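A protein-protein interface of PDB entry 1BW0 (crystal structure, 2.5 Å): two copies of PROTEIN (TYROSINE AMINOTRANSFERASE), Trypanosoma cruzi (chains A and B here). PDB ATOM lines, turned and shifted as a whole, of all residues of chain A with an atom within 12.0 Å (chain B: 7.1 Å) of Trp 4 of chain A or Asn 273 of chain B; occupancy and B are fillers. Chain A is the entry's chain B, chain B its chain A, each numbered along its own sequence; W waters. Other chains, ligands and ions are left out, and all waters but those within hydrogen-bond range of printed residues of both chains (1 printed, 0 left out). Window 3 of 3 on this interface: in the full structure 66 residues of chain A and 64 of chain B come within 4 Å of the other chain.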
ATOM      1  N   TRP A   4     -29.771   7.159  -6.612  1.00  0.00           N
ATOM      2  CA  TRP A   4     -29.657   8.092  -7.725  1.00  0.00           C
ATOM      3  C   TRP A   4     -31.000   8.674  -8.151  1.00  0.00           C
ATOM      4  O   TRP A   4     -31.749   8.023  -8.882  1.00  0.00           O
ATOM      5  CB  TRP A   4     -29.005   7.455  -8.959  1.00  0.00           C
ATOM      6  CG  TRP A   4     -27.511   7.415  -8.894  1.00  0.00           C
ATOM      7  CD1 TRP A   4     -26.735   6.299  -8.771  1.00  0.00           C
ATOM      8  CD2 TRP A   4     -26.610   8.528  -8.936  1.00  0.00           C
ATOM      9  NE1 TRP A   4     -25.410   6.653  -8.738  1.00  0.00           N
ATOM     10  CE2 TRP A   4     -25.303   8.016  -8.832  1.00  0.00           C
ATOM     11  CE3 TRP A   4     -26.778   9.913  -9.044  1.00  0.00           C
ATOM     12  CZ2 TRP A   4     -24.171   8.831  -8.834  1.00  0.00           C
ATOM     13  CZ3 TRP A   4     -25.653  10.715  -9.057  1.00  0.00           C
ATOM     14  CH2 TRP A   4     -24.364  10.179  -8.934  1.00  0.00           C
ATOM     15  N   ASP A   5     -31.283   9.909  -7.752  1.00  0.00           N
ATOM     16  CA  ASP A   5     -32.544  10.530  -8.148  1.00  0.00           C
ATOM     17  C   ASP A   5     -32.300  11.815  -8.933  1.00  0.00           C
ATOM     18  O   ASP A   5     -32.246  12.901  -8.367  1.00  0.00           O
ATOM     19  CB  ASP A   5     -33.448  10.784  -6.940  1.00  0.00           C
ATOM     20  CG  ASP A   5     -34.809  11.309  -7.379  1.00  0.00           C
ATOM     21  OD1 ASP A   5     -35.363  10.766  -8.365  1.00  0.00           O
ATOM     22  OD2 ASP A   5     -35.298  12.271  -6.741  1.00  0.00           O
ATOM     23  N   VAL A   6     -32.128  11.686 -10.245  1.00  0.00           N
ATOM     24  CA  VAL A   6     -31.891  12.836 -11.111  1.00  0.00           C
ATOM     25  C   VAL A   6     -33.153  13.094 -11.931  1.00  0.00           C
ATOM     26  O   VAL A   6     -33.513  12.305 -12.804  1.00  0.00           O
ATOM     27  CB  VAL A   6     -30.688  12.643 -12.043  1.00  0.00           C
ATOM     28  CG1 VAL A   6     -30.386  13.922 -12.815  1.00  0.00           C
ATOM     29  CG2 VAL A   6     -29.461  12.202 -11.253  1.00  0.00           C
ATOM     30  N   SER A   7     -33.855  14.165 -11.584  1.00  0.00           N
ATOM     31  CA  SER A   7     -35.090  14.508 -12.284  1.00  0.00           C
ATOM     32  C   SER A   7     -34.938  15.872 -12.945  1.00  0.00           C
ATOM     33  O   SER A   7     -34.290  16.746 -12.362  1.00  0.00           O
ATOM     34  CB  SER A   7     -36.272  14.494 -11.316  1.00  0.00           C
ATOM     35  OG  SER A   7     -36.214  15.596 -10.427  1.00  0.00           O
ATOM     36  N   MET A   8     -35.519  16.052 -14.129  1.00  0.00           N
ATOM     37  CA  MET A   8     -35.392  17.347 -14.802  1.00  0.00           C
ATOM     38  C   MET A   8     -36.159  18.406 -14.025  1.00  0.00           C
ATOM     39  O   MET A   8     -37.039  18.043 -13.244  1.00  0.00           O
ATOM     40  CB  MET A   8     -35.841  17.283 -16.249  1.00  0.00           C
ATOM     41  CG  MET A   8     -37.326  17.169 -16.534  1.00  0.00           C
ATOM     42  SD  MET A   8     -37.608  17.109 -18.314  1.00  0.00           S
ATOM     43  CE  MET A   8     -37.062  15.452 -18.694  1.00  0.00           C
ATOM     44  N   ALA B 206     -18.539  12.973  -5.861  1.00  0.00           N
ATOM     45  CA  ALA B 206     -19.852  13.148  -6.477  1.00  0.00           C
ATOM     46  C   ALA B 206     -20.623  11.829  -6.396  1.00  0.00           C
ATOM     47  O   ALA B 206     -21.785  11.767  -5.994  1.00  0.00           O
ATOM     48  CB  ALA B 206     -19.698  13.626  -7.910  1.00  0.00           C
ATOM     49  N   GLU B 207     -19.933  10.738  -6.715  1.00  0.00           N
ATOM     50  CA  GLU B 207     -20.457   9.385  -6.642  1.00  0.00           C
ATOM     51  C   GLU B 207     -21.030   9.106  -5.258  1.00  0.00           C
ATOM     52  O   GLU B 207     -22.199   8.773  -5.093  1.00  0.00           O
ATOM     53  CB  GLU B 207     -19.330   8.401  -6.939  1.00  0.00           C
ATOM     54  CG  GLU B 207     -19.759   7.036  -7.451  1.00  0.00           C
ATOM     55  CD  GLU B 207     -18.536   6.215  -7.825  1.00  0.00           C
ATOM     56  OE1 GLU B 207     -17.627   6.767  -8.483  1.00  0.00           O
ATOM     57  OE2 GLU B 207     -18.480   5.029  -7.448  1.00  0.00           O
ATOM     58  N   GLU B 208     -20.197   9.308  -4.247  1.00  0.00           N
ATOM     59  CA  GLU B 208     -20.556   9.141  -2.849  1.00  0.00           C
ATOM     60  C   GLU B 208     -21.735  10.007  -2.433  1.00  0.00           C
ATOM     61  O   GLU B 208     -22.639   9.561  -1.726  1.00  0.00           O
ATOM     62  CB  GLU B 208     -19.319   9.473  -2.014  1.00  0.00           C
ATOM     63  CG  GLU B 208     -19.534   9.751  -0.543  1.00  0.00           C
ATOM     64  CD  GLU B 208     -18.209   9.968   0.173  1.00  0.00           C
ATOM     65  OE1 GLU B 208     -17.412   9.002   0.192  1.00  0.00           O
ATOM     66  OE2 GLU B 208     -17.967  11.073   0.698  1.00  0.00           O
ATOM     67  N   LEU B 209     -21.740  11.266  -2.859  1.00  0.00           N
ATOM     68  CA  LEU B 209     -22.780  12.218  -2.523  1.00  0.00           C
ATOM     69  C   LEU B 209     -24.049  12.080  -3.355  1.00  0.00           C
ATOM     70  O   LEU B 209     -25.060  12.720  -3.046  1.00  0.00           O
ATOM     71  CB  LEU B 209     -22.260  13.649  -2.694  1.00  0.00           C
ATOM     72  CG  LEU B 209     -21.305  14.234  -1.663  1.00  0.00           C
ATOM     73  CD1 LEU B 209     -21.103  15.715  -1.962  1.00  0.00           C
ATOM     74  CD2 LEU B 209     -21.818  14.056  -0.245  1.00  0.00           C
ATOM     75  N   ARG B 210     -23.983  11.326  -4.447  1.00  0.00           N
ATOM     76  CA  ARG B 210     -25.123  11.131  -5.333  1.00  0.00           C
ATOM     77  C   ARG B 210     -25.550  12.434  -6.008  1.00  0.00           C
ATOM     78  O   ARG B 210     -26.729  12.728  -6.212  1.00  0.00           O
ATOM     79  CB  ARG B 210     -26.282  10.471  -4.586  1.00  0.00           C
ATOM     80  CG  ARG B 210     -26.056   9.044  -4.117  1.00  0.00           C
ATOM     81  CD  ARG B 210     -26.065   8.084  -5.285  1.00  0.00           C
ATOM     82  NE  ARG B 210     -26.151   6.685  -4.935  1.00  0.00           N
ATOM     83  CZ  ARG B 210     -25.214   5.767  -4.742  1.00  0.00           C
ATOM     84  NH1 ARG B 210     -23.916   6.031  -4.862  1.00  0.00           N
ATOM     85  NH2 ARG B 210     -25.586   4.524  -4.435  1.00  0.00           N
ATOM     86  N   LEU B 211     -24.565  13.191  -6.490  1.00  0.00           N
ATOM     87  CA  LEU B 211     -24.791  14.421  -7.221  1.00  0.00           C
ATOM     88  C   LEU B 211     -24.303  14.284  -8.672  1.00  0.00           C
ATOM     89  O   LEU B 211     -23.191  13.815  -8.913  1.00  0.00           O
ATOM     90  CB  LEU B 211     -24.014  15.592  -6.648  1.00  0.00           C
ATOM     91  CG  LEU B 211     -24.278  16.221  -5.303  1.00  0.00           C
ATOM     92  CD1 LEU B 211     -23.062  17.067  -4.919  1.00  0.00           C
ATOM     93  CD2 LEU B 211     -25.515  17.101  -5.300  1.00  0.00           C
ATOM     94  N   PRO B 212     -25.124  14.733  -9.611  1.00  0.00           N
ATOM     95  CA  PRO B 212     -24.739  14.758 -11.015  1.00  0.00           C
ATOM     96  C   PRO B 212     -23.640  15.808 -11.125  1.00  0.00           C
ATOM     97  O   PRO B 212     -23.563  16.677 -10.250  1.00  0.00           O
ATOM     98  CB  PRO B 212     -26.011  15.129 -11.743  1.00  0.00           C
ATOM     99  CG  PRO B 212     -26.844  15.863 -10.757  1.00  0.00           C
ATOM    100  CD  PRO B 212     -26.450  15.348  -9.399  1.00  0.00           C
ATOM    101  N   LEU B 213     -22.780  15.740 -12.129  1.00  0.00           N
ATOM    102  CA  LEU B 213     -21.660  16.670 -12.198  1.00  0.00           C
ATOM    103  C   LEU B 213     -21.583  17.490 -13.473  1.00  0.00           C
ATOM    104  O   LEU B 213     -21.537  16.947 -14.575  1.00  0.00           O
ATOM    105  CB  LEU B 213     -20.372  15.849 -12.047  1.00  0.00           C
ATOM    106  CG  LEU B 213     -19.058  16.602 -11.852  1.00  0.00           C
ATOM    107  CD1 LEU B 213     -19.077  17.349 -10.530  1.00  0.00           C
ATOM    108  CD2 LEU B 213     -17.891  15.625 -11.921  1.00  0.00           C
ATOM    109  N   THR B 241     -17.070   5.560 -13.905  1.00  0.00           N
ATOM    110  CA  THR B 241     -17.881   5.991 -12.773  1.00  0.00           C
ATOM    111  C   THR B 241     -19.370   5.933 -13.068  1.00  0.00           C
ATOM    112  O   THR B 241     -19.804   5.942 -14.219  1.00  0.00           O
ATOM    113  CB  THR B 241     -17.499   7.403 -12.290  1.00  0.00           C
ATOM    114  OG1 THR B 241     -18.302   7.744 -11.150  1.00  0.00           O
ATOM    115  CG2 THR B 241     -17.688   8.451 -13.375  1.00  0.00           C
ATOM    116  N   THR B 242     -20.170   5.923 -12.001  1.00  0.00           N
ATOM    117  CA  THR B 242     -21.618   5.881 -12.119  1.00  0.00           C
ATOM    118  C   THR B 242     -22.230   7.278 -12.065  1.00  0.00           C
ATOM    119  O   THR B 242     -23.449   7.445 -11.976  1.00  0.00           O
ATOM    120  CB  THR B 242     -22.251   5.066 -10.972  1.00  0.00           C
ATOM    121  OG1 THR B 242     -21.902   5.733  -9.751  1.00  0.00           O
ATOM    122  CG2 THR B 242     -21.750   3.634 -10.951  1.00  0.00           C
ATOM    123  N   VAL B 243     -21.378   8.300 -12.028  1.00  0.00           N
ATOM    124  CA  VAL B 243     -21.854   9.670 -11.983  1.00  0.00           C
ATOM    125  C   VAL B 243     -22.259  10.171 -13.367  1.00  0.00           C
ATOM    126  O   VAL B 243     -21.521  10.111 -14.351  1.00  0.00           O
ATOM    127  CB  VAL B 243     -20.793  10.626 -11.405  1.00  0.00           C
ATOM    128  CG1 VAL B 243     -21.310  12.062 -11.362  1.00  0.00           C
ATOM    129  CG2 VAL B 243     -20.366  10.179 -10.014  1.00  0.00           C
ATOM    130  N   PRO B 244     -23.474  10.695 -13.430  1.00  0.00           N
ATOM    131  CA  PRO B 244     -23.977  11.319 -14.648  1.00  0.00           C
ATOM    132  C   PRO B 244     -23.240  12.657 -14.782  1.00  0.00           C
ATOM    133  O   PRO B 244     -23.199  13.458 -13.845  1.00  0.00           O
ATOM    134  CB  PRO B 244     -25.459  11.457 -14.409  1.00  0.00           C
ATOM    135  CG  PRO B 244     -25.744  11.042 -13.007  1.00  0.00           C
ATOM    136  CD  PRO B 244     -24.433  10.835 -12.312  1.00  0.00           C
ATOM    137  N   TYR B 267     -22.940  15.066 -22.500  1.00  0.00           N
ATOM    138  CA  TYR B 267     -23.428  14.272 -21.372  1.00  0.00           C
ATOM    139  C   TYR B 267     -22.797  12.890 -21.450  1.00  0.00           C
ATOM    140  O   TYR B 267     -22.771  12.232 -22.479  1.00  0.00           O
ATOM    141  CB  TYR B 267     -24.943  14.264 -21.376  1.00  0.00           C
ATOM    142  CG  TYR B 267     -25.723  13.115 -20.809  1.00  0.00           C
ATOM    143  CD1 TYR B 267     -25.855  11.936 -21.541  1.00  0.00           C
ATOM    144  CD2 TYR B 267     -26.375  13.191 -19.587  1.00  0.00           C
ATOM    145  CE1 TYR B 267     -26.584  10.860 -21.064  1.00  0.00           C
ATOM    146  CE2 TYR B 267     -27.109  12.130 -19.094  1.00  0.00           C
ATOM    147  CZ  TYR B 267     -27.212  10.969 -19.840  1.00  0.00           C
ATOM    148  OH  TYR B 267     -27.925   9.889 -19.362  1.00  0.00           O
ATOM    149  N   ASP B 269     -22.910   9.435 -19.263  1.00  0.00           N
ATOM    150  CA  ASP B 269     -23.631   8.666 -18.253  1.00  0.00           C
ATOM    151  C   ASP B 269     -23.903   7.270 -18.789  1.00  0.00           C
ATOM    152  O   ASP B 269     -25.028   6.896 -19.107  1.00  0.00           O
ATOM    153  CB  ASP B 269     -24.928   9.396 -17.928  1.00  0.00           C
ATOM    154  CG  ASP B 269     -25.787   8.753 -16.859  1.00  0.00           C
ATOM    155  OD1 ASP B 269     -25.261   7.867 -16.143  1.00  0.00           O
ATOM    156  OD2 ASP B 269     -26.979   9.144 -16.764  1.00  0.00           O
ATOM    157  N   PRO B 270     -22.855   6.467 -18.940  1.00  0.00           N
ATOM    158  CA  PRO B 270     -22.936   5.135 -19.511  1.00  0.00           C
ATOM    159  C   PRO B 270     -23.803   4.146 -18.755  1.00  0.00           C
ATOM    160  O   PRO B 270     -24.403   3.247 -19.351  1.00  0.00           O
ATOM    161  CB  PRO B 270     -21.491   4.661 -19.577  1.00  0.00           C
ATOM    162  CG  PRO B 270     -20.651   5.875 -19.413  1.00  0.00           C
ATOM    163  CD  PRO B 270     -21.457   6.830 -18.576  1.00  0.00           C
ATOM    164  N   HIS B 271     -23.924   4.300 -17.445  1.00  0.00           N
ATOM    165  CA  HIS B 271     -24.727   3.455 -16.586  1.00  0.00           C
ATOM    166  C   HIS B 271     -26.135   3.998 -16.369  1.00  0.00           C
ATOM    167  O   HIS B 271     -26.841   3.571 -15.452  1.00  0.00           O
ATOM    168  CB  HIS B 271     -24.038   3.287 -15.223  1.00  0.00           C
ATOM    169  CG  HIS B 271     -22.691   2.638 -15.260  1.00  0.00           C
ATOM    170  ND1 HIS B 271     -22.501   1.298 -14.992  1.00  0.00           N
ATOM    171  CD2 HIS B 271     -21.458   3.139 -15.519  1.00  0.00           C
ATOM    172  CE1 HIS B 271     -21.211   1.005 -15.086  1.00  0.00           C
ATOM    173  NE2 HIS B 271     -20.553   2.107 -15.409  1.00  0.00           N
ATOM    174  N   GLY B 272     -26.558   4.968 -17.165  1.00  0.00           N
ATOM    175  CA  GLY B 272     -27.851   5.588 -17.128  1.00  0.00           C
ATOM    176  C   GLY B 272     -28.402   5.982 -15.780  1.00  0.00           C
ATOM    177  O   GLY B 272     -29.562   5.669 -15.490  1.00  0.00           O
ATOM    178  N   ASN B 273     -27.690   6.781 -14.994  1.00  0.00           N
ATOM    179  CA  ASN B 273     -28.192   7.210 -13.698  1.00  0.00           C
ATOM    180  C   ASN B 273     -28.856   8.576 -13.736  1.00  0.00           C
ATOM    181  O   ASN B 273     -29.442   9.005 -12.735  1.00  0.00           O
ATOM    182  CB  ASN B 273     -27.080   7.167 -12.647  1.00  0.00           C
ATOM    183  CG  ASN B 273     -26.812   5.755 -12.158  1.00  0.00           C
ATOM    184  OD1 ASN B 273     -27.751   4.987 -11.933  1.00  0.00           O
ATOM    185  ND2 ASN B 273     -25.547   5.402 -11.985  1.00  0.00           N
ATOM    186  N   GLY B 274     -28.821   9.262 -14.877  1.00  0.00           N
ATOM    187  CA  GLY B 274     -29.468  10.570 -14.954  1.00  0.00           C
ATOM    188  C   GLY B 274     -29.900  10.975 -16.346  1.00  0.00           C
ATOM    189  O   GLY B 274     -29.570  12.067 -16.811  1.00  0.00           O
ATOM    190  N   PRO B 275     -30.680  10.133 -17.015  1.00  0.00           N
ATOM    191  CA  PRO B 275     -31.167  10.397 -18.358  1.00  0.00           C
ATOM    192  C   PRO B 275     -32.061  11.615 -18.467  1.00  0.00           C
ATOM    193  O   PRO B 275     -32.088  12.272 -19.511  1.00  0.00           O
ATOM    194  CB  PRO B 275     -31.876   9.112 -18.775  1.00  0.00           C
ATOM    195  CG  PRO B 275     -32.192   8.406 -17.511  1.00  0.00           C
ATOM    196  CD  PRO B 275     -31.134   8.812 -16.522  1.00  0.00           C
ATOM    197  N   SER B 276     -32.774  11.991 -17.410  1.00  0.00           N
ATOM    198  CA  SER B 276     -33.612  13.171 -17.377  1.00  0.00           C
ATOM    199  C   SER B 276     -32.753  14.427 -17.559  1.00  0.00           C
ATOM    200  O   SER B 276     -33.262  15.419 -18.074  1.00  0.00           O
ATOM    201  CB  SER B 276     -34.375  13.346 -16.063  1.00  0.00           C
ATOM    202  OG  SER B 276     -35.361  12.356 -15.885  1.00  0.00           O
HETATM  203  O   HOH W   1     -31.901   9.228 -11.543  1.00  0.00           O
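ND2 of Asn 273 of chain B lies close to NE1 of Trp 4 of chain A (3.5 Å).
The backbone carbonyl oxygen of Ala 206 of chain B is in hydrogen-bond range of the backbone NH of Leu 211 of chain B (3.2 Å).
The backbone carbonyl oxygen of Glu 207 of chain B lies within hydrogen-bond range of the guanidinium group of Arg 210 of chain B, at 3.2 Å.
N of Leu 213 of chain B lies within hydrogen-bond range of O of Pro 244 of chain B (2.9 Å).
The backbone NH (N) of Val 243 of chain B sits at hydrogen-bond distance from the side-chain hydroxyl (OG1) of Thr 241 of chain B (3.2 Å).
The backbone carbonyl oxygen of Thr 242 of chain B is in hydrogen-bond range of the side-chain amide nitrogen of Asn 273 of chain B (2.9 Å).
The backbone NH (N) of Asn 273 of chain B sits at hydrogen-bond distance from the side-chain carboxylate (OD1) of Asp 269 of chain B.
Trp 4 of chain A touches Arg 210 of chain B.
Leu 211 of chain B touches Trp 4 of chain A.
CZ2 of Trp 4 of chain A touches O of Thr 242 of chain B (3.5 Å).
CH2 of Trp 4 of chain A touches CA of Val 243 of chain B (3.98 Å).
Trp 4 of chain A touches Pro 244 of chain B (CH2 to CD, 3.4 Å).
Val 6 of chain A touches Asn 273 of chain B.
CB of Val 6 of chain A touches CA of Gly 274 of chain B, 3.8 Å away.
Ser 276 of chain B touches Val 6 of chain A.
N of Met 8 of chain A touches CB of Ser 276 of chain B (3.5 Å).
Of the printed residues of chain B, Trp 4 of chain A touches Arg 210, Leu 211, Thr 242, Val 243, Pro 244 and Asn 273.
Printed residues of chain A within 4 Å of Asn 273 of chain B: Trp 4 (3.4 Å) and Val 6 (3.5 Å).
No residue of chain A comes within 4 Å of Pro 212 of chain B.
Thr 242 of chain B touches just one residue of chain A: Trp 4 (3.5 Å).
Pro 244 of chain B touches just one residue of chain A: Trp 4.
No residue of chain A comes within 4 Å of Asp 269 of chain B.
No residue of chain A comes within 4 Å of His 271 of chain B.
Gly 274 of chain B touches one residue of chain A.
No residue of chain A comes within 4 Å of Pro 275 of chain B.
Of the printed residues of chain A, Ser 276 of chain B touches Val 6 and Met 8.
Of the printed residues of chain A, Val 243 of chain B touches Trp 4 (3.98 Å).
Printed residues of chain B within 4 Å of Met 8 of chain A: Ser 276 (3.5 Å).
Printed residues of chain B within 4 Å of Val 6 of chain A: Asn 273, Gly 274 and Ser 276.
Printed residues of chain A within 4 Å of Leu 211 of chain B: Trp 4.
Leu 209 of chain B touches none of the printed residues of chain A.
Thr 241 of chain B touches none of the printed residues of chain A.
The nearest residue of chain A that does not touch Asn 273 of chain B is Asp 5 of chain A (5.4 Å).
The nearest printed residue of chain B that does not touch Val 6 of chain A is Pro 244 of chain B (4.3 Å).
Of the 21 printed residues of chain B, 8 touch a printed residue of chain A.
Of the 5 printed residues of chain A, 3 touch a printed residue of chain B.
Printed residues of chain A that touch a printed residue of chain B: Trp 4, Val 6 and Met 8.
Hydrophobic or aromatic side chains of chain A within 4 Å of the printed part of chain B: Trp 4, Val 6 and Met 8.
Among the printed residues, no Asp or Glu carboxylate lies within 4 Å of a Lys or Arg side-chain nitrogen of the other chain.
No position is printed for both chains.
Water W1 lies within hydrogen-bond range of O of Asn 273 of chain B, N of Val 6 of chain A and O of Trp 4 of chain A.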
